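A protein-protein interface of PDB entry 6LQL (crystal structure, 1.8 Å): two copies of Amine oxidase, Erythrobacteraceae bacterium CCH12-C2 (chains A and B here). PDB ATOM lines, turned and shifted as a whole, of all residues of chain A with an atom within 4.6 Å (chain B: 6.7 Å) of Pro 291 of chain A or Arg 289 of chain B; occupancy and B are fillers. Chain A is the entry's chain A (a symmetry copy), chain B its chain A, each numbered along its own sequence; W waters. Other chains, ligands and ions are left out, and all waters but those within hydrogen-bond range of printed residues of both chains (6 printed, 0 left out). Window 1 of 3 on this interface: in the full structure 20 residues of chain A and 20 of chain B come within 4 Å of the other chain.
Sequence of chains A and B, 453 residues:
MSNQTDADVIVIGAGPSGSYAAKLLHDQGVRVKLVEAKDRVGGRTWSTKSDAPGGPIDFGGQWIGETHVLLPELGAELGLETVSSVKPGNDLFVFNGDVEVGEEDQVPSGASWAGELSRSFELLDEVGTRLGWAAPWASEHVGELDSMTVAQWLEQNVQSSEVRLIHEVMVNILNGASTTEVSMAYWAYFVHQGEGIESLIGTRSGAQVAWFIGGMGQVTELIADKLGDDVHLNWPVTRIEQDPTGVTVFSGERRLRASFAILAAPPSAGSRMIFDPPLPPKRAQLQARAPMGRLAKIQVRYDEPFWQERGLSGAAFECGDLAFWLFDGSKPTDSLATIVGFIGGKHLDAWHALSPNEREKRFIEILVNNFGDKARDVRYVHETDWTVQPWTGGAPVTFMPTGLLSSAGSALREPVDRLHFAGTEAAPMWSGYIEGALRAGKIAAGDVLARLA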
ATOM      1  N   GLU A 181      10.803  31.237  15.703  1.00  0.00           N
ATOM      2  CA  GLU A 181       9.423  30.924  16.058  1.00  0.00           C
ATOM      3  C   GLU A 181       8.913  31.707  17.256  1.00  0.00           C
ATOM      4  O   GLU A 181       7.704  31.948  17.347  1.00  0.00           O
ATOM      5  CB  GLU A 181       9.292  29.426  16.368  1.00  0.00           C
ATOM      6  CG  GLU A 181       9.539  28.552  15.155  1.00  0.00           C
ATOM      7  CD  GLU A 181       9.844  27.073  15.501  1.00  0.00           C
ATOM      8  OE1 GLU A 181       9.902  26.707  16.696  1.00  0.00           O
ATOM      9  OE2 GLU A 181      10.022  26.273  14.553  1.00  0.00           O
ATOM     10  N   ARG A 289      -3.245  29.605  20.687  1.00  0.00           N
ATOM     11  CA  ARG A 289      -2.069  30.113  19.982  1.00  0.00           C
ATOM     12  C   ARG A 289      -0.766  30.079  20.785  1.00  0.00           C
ATOM     13  O   ARG A 289       0.290  30.434  20.235  1.00  0.00           O
ATOM     14  CB  ARG A 289      -2.363  31.534  19.467  1.00  0.00           C
ATOM     15  CG  ARG A 289      -3.347  31.525  18.286  1.00  0.00           C
ATOM     16  CD  ARG A 289      -4.050  32.862  18.030  1.00  0.00           C
ATOM     17  NE  ARG A 289      -3.120  33.985  17.970  1.00  0.00           N
ATOM     18  CZ  ARG A 289      -3.473  35.246  18.194  1.00  0.00           C
ATOM     19  NH1 ARG A 289      -4.739  35.551  18.477  1.00  0.00           N
ATOM     20  NH2 ARG A 289      -2.553  36.202  18.130  1.00  0.00           N
ATOM     21  N   ALA A 290      -0.790  29.603  22.030  1.00  0.00           N
ATOM     22  CA  ALA A 290       0.404  29.427  22.847  1.00  0.00           C
ATOM     23  C   ALA A 290       0.767  27.942  22.867  1.00  0.00           C
ATOM     24  O   ALA A 290       0.277  27.203  23.725  1.00  0.00           O
ATOM     25  CB  ALA A 290       0.160  29.956  24.261  1.00  0.00           C
ATOM     26  N   PRO A 291       1.598  27.458  21.958  1.00  0.00           N
ATOM     27  CA  PRO A 291       1.899  26.022  21.896  1.00  0.00           C
ATOM     28  C   PRO A 291       2.954  25.593  22.911  1.00  0.00           C
ATOM     29  O   PRO A 291       3.684  26.397  23.478  1.00  0.00           O
ATOM     30  CB  PRO A 291       2.436  25.835  20.467  1.00  0.00           C
ATOM     31  CG  PRO A 291       2.480  27.236  19.842  1.00  0.00           C
ATOM     32  CD  PRO A 291       2.346  28.220  20.956  1.00  0.00           C
ATOM     33  N   MET A 292       3.030  24.276  23.110  1.00  0.00           N
ATOM     34  CA  MET A 292       4.188  23.706  23.780  1.00  0.00           C
ATOM     35  C   MET A 292       5.417  23.758  22.867  1.00  0.00           C
ATOM     36  O   MET A 292       5.343  23.591  21.644  1.00  0.00           O
ATOM     37  CB  MET A 292       3.925  22.250  24.194  1.00  0.00           C
ATOM     38  CG  MET A 292       2.773  22.044  25.149  1.00  0.00           C
ATOM     39  SD  MET A 292       3.005  22.921  26.704  1.00  0.00           S
ATOM     40  CE  MET A 292       4.546  22.240  27.297  1.00  0.00           C
ATOM     41  N   GLY A 293       6.559  23.984  23.482  1.00  0.00           N
ATOM     42  CA  GLY A 293       7.810  23.766  22.799  1.00  0.00           C
ATOM     43  C   GLY A 293       8.005  22.282  22.567  1.00  0.00           C
ATOM     44  O   GLY A 293       7.177  21.450  22.947  1.00  0.00           O
ATOM     45  N   ARG A 294       9.133  21.941  21.941  1.00  0.00           N
ATOM     46  CA  ARG A 294       9.462  20.535  21.718  1.00  0.00           C
ATOM     47  C   ARG A 294      10.851  20.222  22.262  1.00  0.00           C
ATOM     48  O   ARG A 294      11.805  20.973  22.024  1.00  0.00           O
ATOM     49  CB  ARG A 294       9.353  20.171  20.233  1.00  0.00           C
ATOM     50  CG  ARG A 294      10.065  21.118  19.280  1.00  0.00           C
ATOM     51  CD  ARG A 294       9.359  21.173  17.919  1.00  0.00           C
ATOM     52  NE  ARG A 294      10.121  21.910  16.904  1.00  0.00           N
ATOM     53  CZ  ARG A 294      10.132  23.241  16.785  1.00  0.00           C
ATOM     54  NH1 ARG A 294       9.424  24.017  17.610  1.00  0.00           N
ATOM     55  NH2 ARG A 294      10.844  23.803  15.821  1.00  0.00           N
ATOM     56  N   VAL A 397       8.349  23.901  28.172  1.00  0.00           N
ATOM     57  CA  VAL A 397       7.437  24.984  28.530  1.00  0.00           C
ATOM     58  C   VAL A 397       6.531  25.339  27.355  1.00  0.00           C
ATOM     59  O   VAL A 397       6.774  24.955  26.209  1.00  0.00           O
ATOM     60  CB  VAL A 397       8.211  26.255  28.974  1.00  0.00           C
ATOM     61  CG1 VAL A 397       9.144  25.938  30.130  1.00  0.00           C
ATOM     62  CG2 VAL A 397       9.016  26.826  27.806  1.00  0.00           C
ATOM     63  N   THR A 398       5.490  26.112  27.660  1.00  0.00           N
ATOM     64  CA  THR A 398       4.733  26.859  26.663  1.00  0.00           C
ATOM     65  C   THR A 398       5.589  28.002  26.114  1.00  0.00           C
ATOM     66  O   THR A 398       6.344  28.626  26.859  1.00  0.00           O
ATOM     67  CB  THR A 398       3.478  27.443  27.327  1.00  0.00           C
ATOM     68  OG1 THR A 398       2.598  26.387  27.747  1.00  0.00           O
ATOM     69  CG2 THR A 398       2.732  28.414  26.418  1.00  0.00           C
ATOM     70  N   PHE A 399       5.467  28.286  24.819  1.00  0.00           N
ATOM     71  CA  PHE A 399       6.059  29.499  24.249  1.00  0.00           C
ATOM     72  C   PHE A 399       4.991  30.275  23.494  1.00  0.00           C
ATOM     73  O   PHE A 399       3.862  29.812  23.317  1.00  0.00           O
ATOM     74  CB  PHE A 399       7.254  29.196  23.316  1.00  0.00           C
ATOM     75  CG  PHE A 399       6.871  28.653  21.946  1.00  0.00           C
ATOM     76  CD1 PHE A 399       6.668  27.303  21.752  1.00  0.00           C
ATOM     77  CD2 PHE A 399       6.768  29.490  20.845  1.00  0.00           C
ATOM     78  CE1 PHE A 399       6.339  26.808  20.502  1.00  0.00           C
ATOM     79  CE2 PHE A 399       6.443  28.992  19.582  1.00  0.00           C
ATOM     80  CZ  PHE A 399       6.233  27.646  19.416  1.00  0.00           C
ATOM     81  N   PRO A 401       4.311  32.790  19.871  1.00  0.00           N
ATOM     82  CA  PRO A 401       4.822  33.411  18.641  1.00  0.00           C
ATOM     83  C   PRO A 401       4.507  34.899  18.622  1.00  0.00           C
ATOM     84  O   PRO A 401       3.883  35.400  19.566  1.00  0.00           O
ATOM     85  CB  PRO A 401       4.059  32.679  17.534  1.00  0.00           C
ATOM     86  CG  PRO A 401       2.691  32.455  18.182  1.00  0.00           C
ATOM     87  CD  PRO A 401       2.980  32.172  19.661  1.00  0.00           C
ATOM     88  N   SER B 271      -5.314  18.489  16.452  1.00  0.00           N
ATOM     89  CA  SER B 271      -4.464  18.641  17.628  1.00  0.00           C
ATOM     90  C   SER B 271      -5.182  18.265  18.919  1.00  0.00           C
ATOM     91  O   SER B 271      -4.517  17.951  19.911  1.00  0.00           O
ATOM     92  CB  SER B 271      -3.951  20.084  17.732  1.00  0.00           C
ATOM     93  OG  SER B 271      -5.022  20.942  18.116  1.00  0.00           O
ATOM     94  N   ALA B 284       2.415  16.241  13.837  1.00  0.00           N
ATOM     95  CA  ALA B 284       2.072  16.672  15.189  1.00  0.00           C
ATOM     96  C   ALA B 284       2.331  18.169  15.380  1.00  0.00           C
ATOM     97  O   ALA B 284       1.493  18.895  15.948  1.00  0.00           O
ATOM     98  CB  ALA B 284       2.861  15.864  16.216  1.00  0.00           C
ATOM     99  N   GLN B 285       3.492  18.645  14.916  1.00  0.00           N
ATOM    100  CA  GLN B 285       3.807  20.073  15.034  1.00  0.00           C
ATOM    101  C   GLN B 285       2.844  20.931  14.220  1.00  0.00           C
ATOM    102  O   GLN B 285       2.396  21.996  14.678  1.00  0.00           O
ATOM    103  CB  GLN B 285       5.251  20.322  14.596  1.00  0.00           C
ATOM    104  CG  GLN B 285       6.302  19.794  15.587  1.00  0.00           C
ATOM    105  CD  GLN B 285       6.096  20.314  16.988  1.00  0.00           C
ATOM    106  OE1 GLN B 285       5.981  21.521  17.218  1.00  0.00           O
ATOM    107  NE2 GLN B 285       6.046  19.405  17.936  1.00  0.00           N
ATOM    108  N   LEU B 286       2.518  20.487  13.006  1.00  0.00           N
ATOM    109  CA  LEU B 286       1.595  21.238  12.165  1.00  0.00           C
ATOM    110  C   LEU B 286       0.254  21.411  12.857  1.00  0.00           C
ATOM    111  O   LEU B 286      -0.299  22.518  12.902  1.00  0.00           O
ATOM    112  CB  LEU B 286       1.424  20.522  10.824  1.00  0.00           C
ATOM    113  CG  LEU B 286       0.475  21.175   9.818  1.00  0.00           C
ATOM    114  CD1 LEU B 286       1.074  22.460   9.295  1.00  0.00           C
ATOM    115  CD2 LEU B 286       0.128  20.213   8.660  1.00  0.00           C
ATOM    116  N   GLN B 287      -0.284  20.322  13.414  1.00  0.00           N
ATOM    117  CA  GLN B 287      -1.586  20.418  14.067  1.00  0.00           C
ATOM    118  C   GLN B 287      -1.531  21.352  15.267  1.00  0.00           C
ATOM    119  O   GLN B 287      -2.477  22.110  15.516  1.00  0.00           O
ATOM    120  CB  GLN B 287      -2.065  19.031  14.496  1.00  0.00           C
ATOM    121  CG  GLN B 287      -2.314  18.131  13.304  1.00  0.00           C
ATOM    122  CD  GLN B 287      -2.980  16.812  13.668  1.00  0.00           C
ATOM    123  OE1 GLN B 287      -3.589  16.193  12.815  1.00  0.00           O
ATOM    124  NE2 GLN B 287      -2.829  16.364  14.913  1.00  0.00           N
ATOM    125  N   ALA B 288      -0.451  21.277  16.049  1.00  0.00           N
ATOM    126  CA  ALA B 288      -0.366  22.089  17.256  1.00  0.00           C
ATOM    127  C   ALA B 288      -0.127  23.574  16.962  1.00  0.00           C
ATOM    128  O   ALA B 288      -0.469  24.432  17.788  1.00  0.00           O
ATOM    129  CB  ALA B 288       0.749  21.545  18.144  1.00  0.00           C
ATOM    130  N   ARG B 289       0.465  23.904  15.818  1.00  0.00           N
ATOM    131  CA  ARG B 289       0.971  25.261  15.621  1.00  0.00           C
ATOM    132  C   ARG B 289       0.332  26.031  14.462  1.00  0.00           C
ATOM    133  O   ARG B 289       0.662  27.213  14.269  1.00  0.00           O
ATOM    134  CB  ARG B 289       2.503  25.212  15.472  1.00  0.00           C
ATOM    135  CG  ARG B 289       3.200  24.904  16.807  1.00  0.00           C
ATOM    136  CD  ARG B 289       4.631  24.374  16.672  1.00  0.00           C
ATOM    137  NE  ARG B 289       5.455  25.196  15.792  1.00  0.00           N
ATOM    138  CZ  ARG B 289       6.543  24.750  15.174  1.00  0.00           C
ATOM    139  NH1 ARG B 289       6.952  23.493  15.351  1.00  0.00           N
ATOM    140  NH2 ARG B 289       7.224  25.568  14.379  1.00  0.00           N
ATOM    141  N   ALA B 290      -0.613  25.433  13.737  1.00  0.00           N
ATOM    142  CA  ALA B 290      -1.362  26.103  12.681  1.00  0.00           C
ATOM    143  C   ALA B 290      -2.753  26.448  13.211  1.00  0.00           C
ATOM    144  O   ALA B 290      -3.670  25.628  13.108  1.00  0.00           O
ATOM    145  CB  ALA B 290      -1.448  25.208  11.443  1.00  0.00           C
ATOM    146  N   PRO B 291      -2.963  27.621  13.788  1.00  0.00           N
ATOM    147  CA  PRO B 291      -4.264  27.948  14.386  1.00  0.00           C
ATOM    148  C   PRO B 291      -5.290  28.409  13.355  1.00  0.00           C
ATOM    149  O   PRO B 291      -4.974  28.765  12.227  1.00  0.00           O
ATOM    150  CB  PRO B 291      -3.929  29.101  15.348  1.00  0.00           C
ATOM    151  CG  PRO B 291      -2.438  29.403  15.149  1.00  0.00           C
ATOM    152  CD  PRO B 291      -2.018  28.736  13.882  1.00  0.00           C
ATOM    153  N   PHE B 399      -4.247  29.659   9.541  1.00  0.00           N
ATOM    154  CA  PHE B 399      -3.057  30.421   9.155  1.00  0.00           C
ATOM    155  C   PHE B 399      -1.832  29.819   9.826  1.00  0.00           C
ATOM    156  O   PHE B 399      -1.933  28.918  10.663  1.00  0.00           O
ATOM    157  CB  PHE B 399      -3.172  31.922   9.509  1.00  0.00           C
ATOM    158  CG  PHE B 399      -2.987  32.244  10.986  1.00  0.00           C
ATOM    159  CD1 PHE B 399      -4.052  32.189  11.859  1.00  0.00           C
ATOM    160  CD2 PHE B 399      -1.759  32.655  11.483  1.00  0.00           C
ATOM    161  CE1 PHE B 399      -3.888  32.501  13.198  1.00  0.00           C
ATOM    162  CE2 PHE B 399      -1.594  32.976  12.832  1.00  0.00           C
ATOM    163  CZ  PHE B 399      -2.665  32.901  13.684  1.00  0.00           C
ATOM    164  N   MET B 400      -0.649  30.323   9.457  1.00  0.00           N
ATOM    165  CA  MET B 400       0.549  29.819  10.111  1.00  0.00           C
ATOM    166  C   MET B 400       1.450  30.972  10.528  1.00  0.00           C
ATOM    167  O   MET B 400       1.588  31.960   9.781  1.00  0.00           O
ATOM    168  CB  MET B 400       1.341  28.881   9.202  1.00  0.00           C
ATOM    169  CG  MET B 400       0.546  27.677   8.748  1.00  0.00           C
ATOM    170  SD  MET B 400       1.629  26.545   7.851  1.00  0.00           S
ATOM    171  CE  MET B 400       0.399  25.344   7.301  1.00  0.00           C
ATOM    172  N   PRO B 401       2.068  30.872  11.723  1.00  0.00           N
ATOM    173  CA  PRO B 401       3.034  31.890  12.160  1.00  0.00           C
ATOM    174  C   PRO B 401       4.417  31.586  11.606  1.00  0.00           C
ATOM    175  O   PRO B 401       4.585  30.580  10.908  1.00  0.00           O
ATOM    176  CB  PRO B 401       3.017  31.758  13.686  1.00  0.00           C
ATOM    177  CG  PRO B 401       2.825  30.251  13.874  1.00  0.00           C
ATOM    178  CD  PRO B 401       1.886  29.814  12.744  1.00  0.00           C
ATOM    179  N   THR B 402       5.412  32.414  11.929  1.00  0.00           N
ATOM    180  CA  THR B 402       6.757  32.187  11.409  1.00  0.00           C
ATOM    181  C   THR B 402       7.265  30.796  11.768  1.00  0.00           C
ATOM    182  O   THR B 402       7.069  30.309  12.887  1.00  0.00           O
ATOM    183  CB  THR B 402       7.737  33.231  11.950  1.00  0.00           C
ATOM    184  OG1 THR B 402       7.697  33.260  13.385  1.00  0.00           O
ATOM    185  CG2 THR B 402       7.393  34.611  11.392  1.00  0.00           C
ATOM    186  N   GLY B 403       7.941  30.170  10.800  1.00  0.00           N
ATOM    187  CA  GLY B 403       8.664  28.947  11.024  1.00  0.00           C
ATOM    188  C   GLY B 403       7.909  27.670  10.728  1.00  0.00           C
ATOM    189  O   GLY B 403       8.549  26.616  10.624  1.00  0.00           O
ATOM    190  N   LEU B 404       6.582  27.722  10.563  1.00  0.00           N
ATOM    191  CA  LEU B 404       5.840  26.461  10.488  1.00  0.00           C
ATOM    192  C   LEU B 404       5.806  25.895   9.073  1.00  0.00           C
ATOM    193  O   LEU B 404       6.111  24.717   8.870  1.00  0.00           O
ATOM    194  CB  LEU B 404       4.408  26.623  11.008  1.00  0.00           C
ATOM    195  CG  LEU B 404       3.679  25.269  11.182  1.00  0.00           C
ATOM    196  CD1 LEU B 404       4.453  24.346  12.137  1.00  0.00           C
ATOM    197  CD2 LEU B 404       2.263  25.524  11.687  1.00  0.00           C
ATOM    198  N   LEU B 405       5.396  26.690   8.083  1.00  0.00           N
ATOM    199  CA  LEU B 405       5.277  26.148   6.729  1.00  0.00           C
ATOM    200  C   LEU B 405       6.584  25.509   6.265  1.00  0.00           C
ATOM    201  O   LEU B 405       6.590  24.386   5.735  1.00  0.00           O
ATOM    202  CB  LEU B 405       4.855  27.251   5.755  1.00  0.00           C
ATOM    203  CG  LEU B 405       4.614  26.854   4.289  1.00  0.00           C
ATOM    204  CD1 LEU B 405       3.387  25.943   4.143  1.00  0.00           C
ATOM    205  CD2 LEU B 405       4.440  28.107   3.424  1.00  0.00           C
ATOM    206  N   SER B 407       8.981  24.209   8.060  1.00  0.00           N
ATOM    207  CA  SER B 407       9.471  23.081   8.850  1.00  0.00           C
ATOM    208  C   SER B 407       8.499  21.913   8.936  1.00  0.00           C
ATOM    209  O   SER B 407       8.935  20.799   9.247  1.00  0.00           O
ATOM    210  CB  SER B 407       9.835  23.521  10.279  1.00  0.00           C
ATOM    211  OG  SER B 407       8.677  23.951  10.991  1.00  0.00           O
ATOM    212  N   ALA B 408       7.224  22.120   8.617  1.00  0.00           N
ATOM    213  CA  ALA B 408       6.221  21.075   8.759  1.00  0.00           C
ATOM    214  C   ALA B 408       5.151  21.097   7.673  1.00  0.00           C
ATOM    215  O   ALA B 408       4.245  20.260   7.736  1.00  0.00           O
ATOM    216  CB  ALA B 408       5.542  21.171  10.151  1.00  0.00           C
HETATM  217  O   HOH W   1       5.660  20.113  20.854  1.00  0.00           O
HETATM  218  O   HOH W   2      11.149  26.509  12.197  1.00  0.00           O
HETATM  219  O   HOH W   3       8.903  22.354  13.438  1.00  0.00           O
HETATM  220  O   HOH W   4       6.637  34.096  15.821  1.00  0.00           O
HETATM  221  O   HOH W   5       6.007  30.524  15.515  1.00  0.00           O
HETATM  222  O   HOH W   6       6.938  23.141  19.361  1.00  0.00           O
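CG of Glu 181 of chain A touches O of Thr 402 of chain B, at 3.8 Å. CG of Arg 289 of chain A touches CB of Pro 291 of chain B, at 3.9 Å. CB of Pro 291 of chain A touches CG of Arg 289 of chain B, at 3.9 Å. Arg 294 of chain A touches Gln 285 of chain B.
Printed residues of chain A that touch a printed residue of chain B: Glu 181, Arg 289, Pro 291 and Arg 294. Hydrophobic or aromatic side chains of chain A that line the printed part of chain B: Pro 291. Along chain A the printed residues that touch a printed residue of chain B span positions 181 to 294. Printed residues of chain B that touch a printed residue of chain A: Gln 285, Arg 289, Pro 291 and Thr 402.
The guanidinium group (NH2) of Arg 289 of chain B is in salt-bridge range of the side-chain carboxylate (OE2) of Glu 181 of chain A (2.9 Å). The guanidinium group (NH1) of Arg 294 of chain A sits close to the guanidinium group (NH1) of Arg 289 of chain B (3.4 Å).
The backbone carbonyl oxygen (O) of Pro 291 of chain B is in hydrogen-bond range of the backbone NH (N) of Phe 399 of chain B, 2.9 Å away. The side-chain carboxylate (OE1) of Glu 181 of chain A lies within salt-bridge range of the guanidinium group (NH1) of Arg 294 of chain A (2.9 Å). The backbone NH (N) of Phe 399 of chain A is in hydrogen-bond range of the backbone carbonyl oxygen (O) of Pro 291 of chain A, at 2.9 Å. The guanidinium group of Arg 289 of chain B is in hydrogen-bond range of the side-chain amide oxygen of Gln 285 of chain B (2.9 Å).
Water W2 lies within hydrogen-bond range of the side-chain carboxylate of Glu 181 of chain A (2.6 Å) and the backbone carbonyl oxygen of Gly 403 of chain B (3.0 Å). Water W4 lies within hydrogen-bond range of the side-chain hydroxyl (OG1) of Thr 402 of chain B (2.8 Å) and the backbone carbonyl oxygen (O) of Glu 181 of chain A (2.8 Å). Water W6 lies within hydrogen-bond range of the backbone carbonyl oxygen of Met 292 of chain A, the side-chain amide oxygen of Gln 285 of chain B and the guanidinium group of Arg 294 of chain A. Water W5 lies within hydrogen-bond range of O of Thr 402 of chain B (2.8 Å) and O of Glu 181 of chain A (2.9 Å). Water W1 lies within hydrogen-bond range of O of Gly 293 of chain A (2.9 Å) and NE2 of Gln 285 of chain B (3.0 Å). Water W3 lies within hydrogen-bond range of the side-chain hydroxyl (OG) of Ser 407 of chain B (2.9 Å), the guanidinium group (NH1) of Arg 289 of chain B (3.0 Å) and the guanidinium group (NH2) of Arg 294 of chain A (3.4 Å).
Arg 289 of chain A touches Pro 291 of chain B, and with the chains exchanged Pro 291 of chain A touches Arg 289 of chain B. Positions printed for both chains: 289, 290, 291, 399 and 401. Of the 6 pairs that touch across the chains among the printed residues, 2 have their exchanged pair printed and touching as well.
Printed residues of chain B within 4 Å of Glu 181 of chain A: Arg 289 (2.9 Å) and Thr 402 (3.8 Å). Printed residues of chain B within 4 Å of Arg 289 of chain A: Pro 291. Of the printed residues of chain A, Gln 285 of chain B touches Arg 294 (3.5 Å). Printed residues of chain A within 4 Å of Arg 289 of chain B: Glu 181 (2.9 Å), Pro 291 (3.9 Å) and Arg 294 (3.4 Å). Of the printed residues of chain A, Pro 291 of chain B touches Arg 289. Printed residues of chain A within 4 Å of Thr 402 of chain B: Glu 181 (3.8 Å). The nearest residue of chain B that does not touch Pro 291 of chain A is Ala 288 of chain B (4.2 Å). The nearest residue of chain A that does not touch Arg 289 of chain B is Phe 399 of chain A (4.4 Å).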
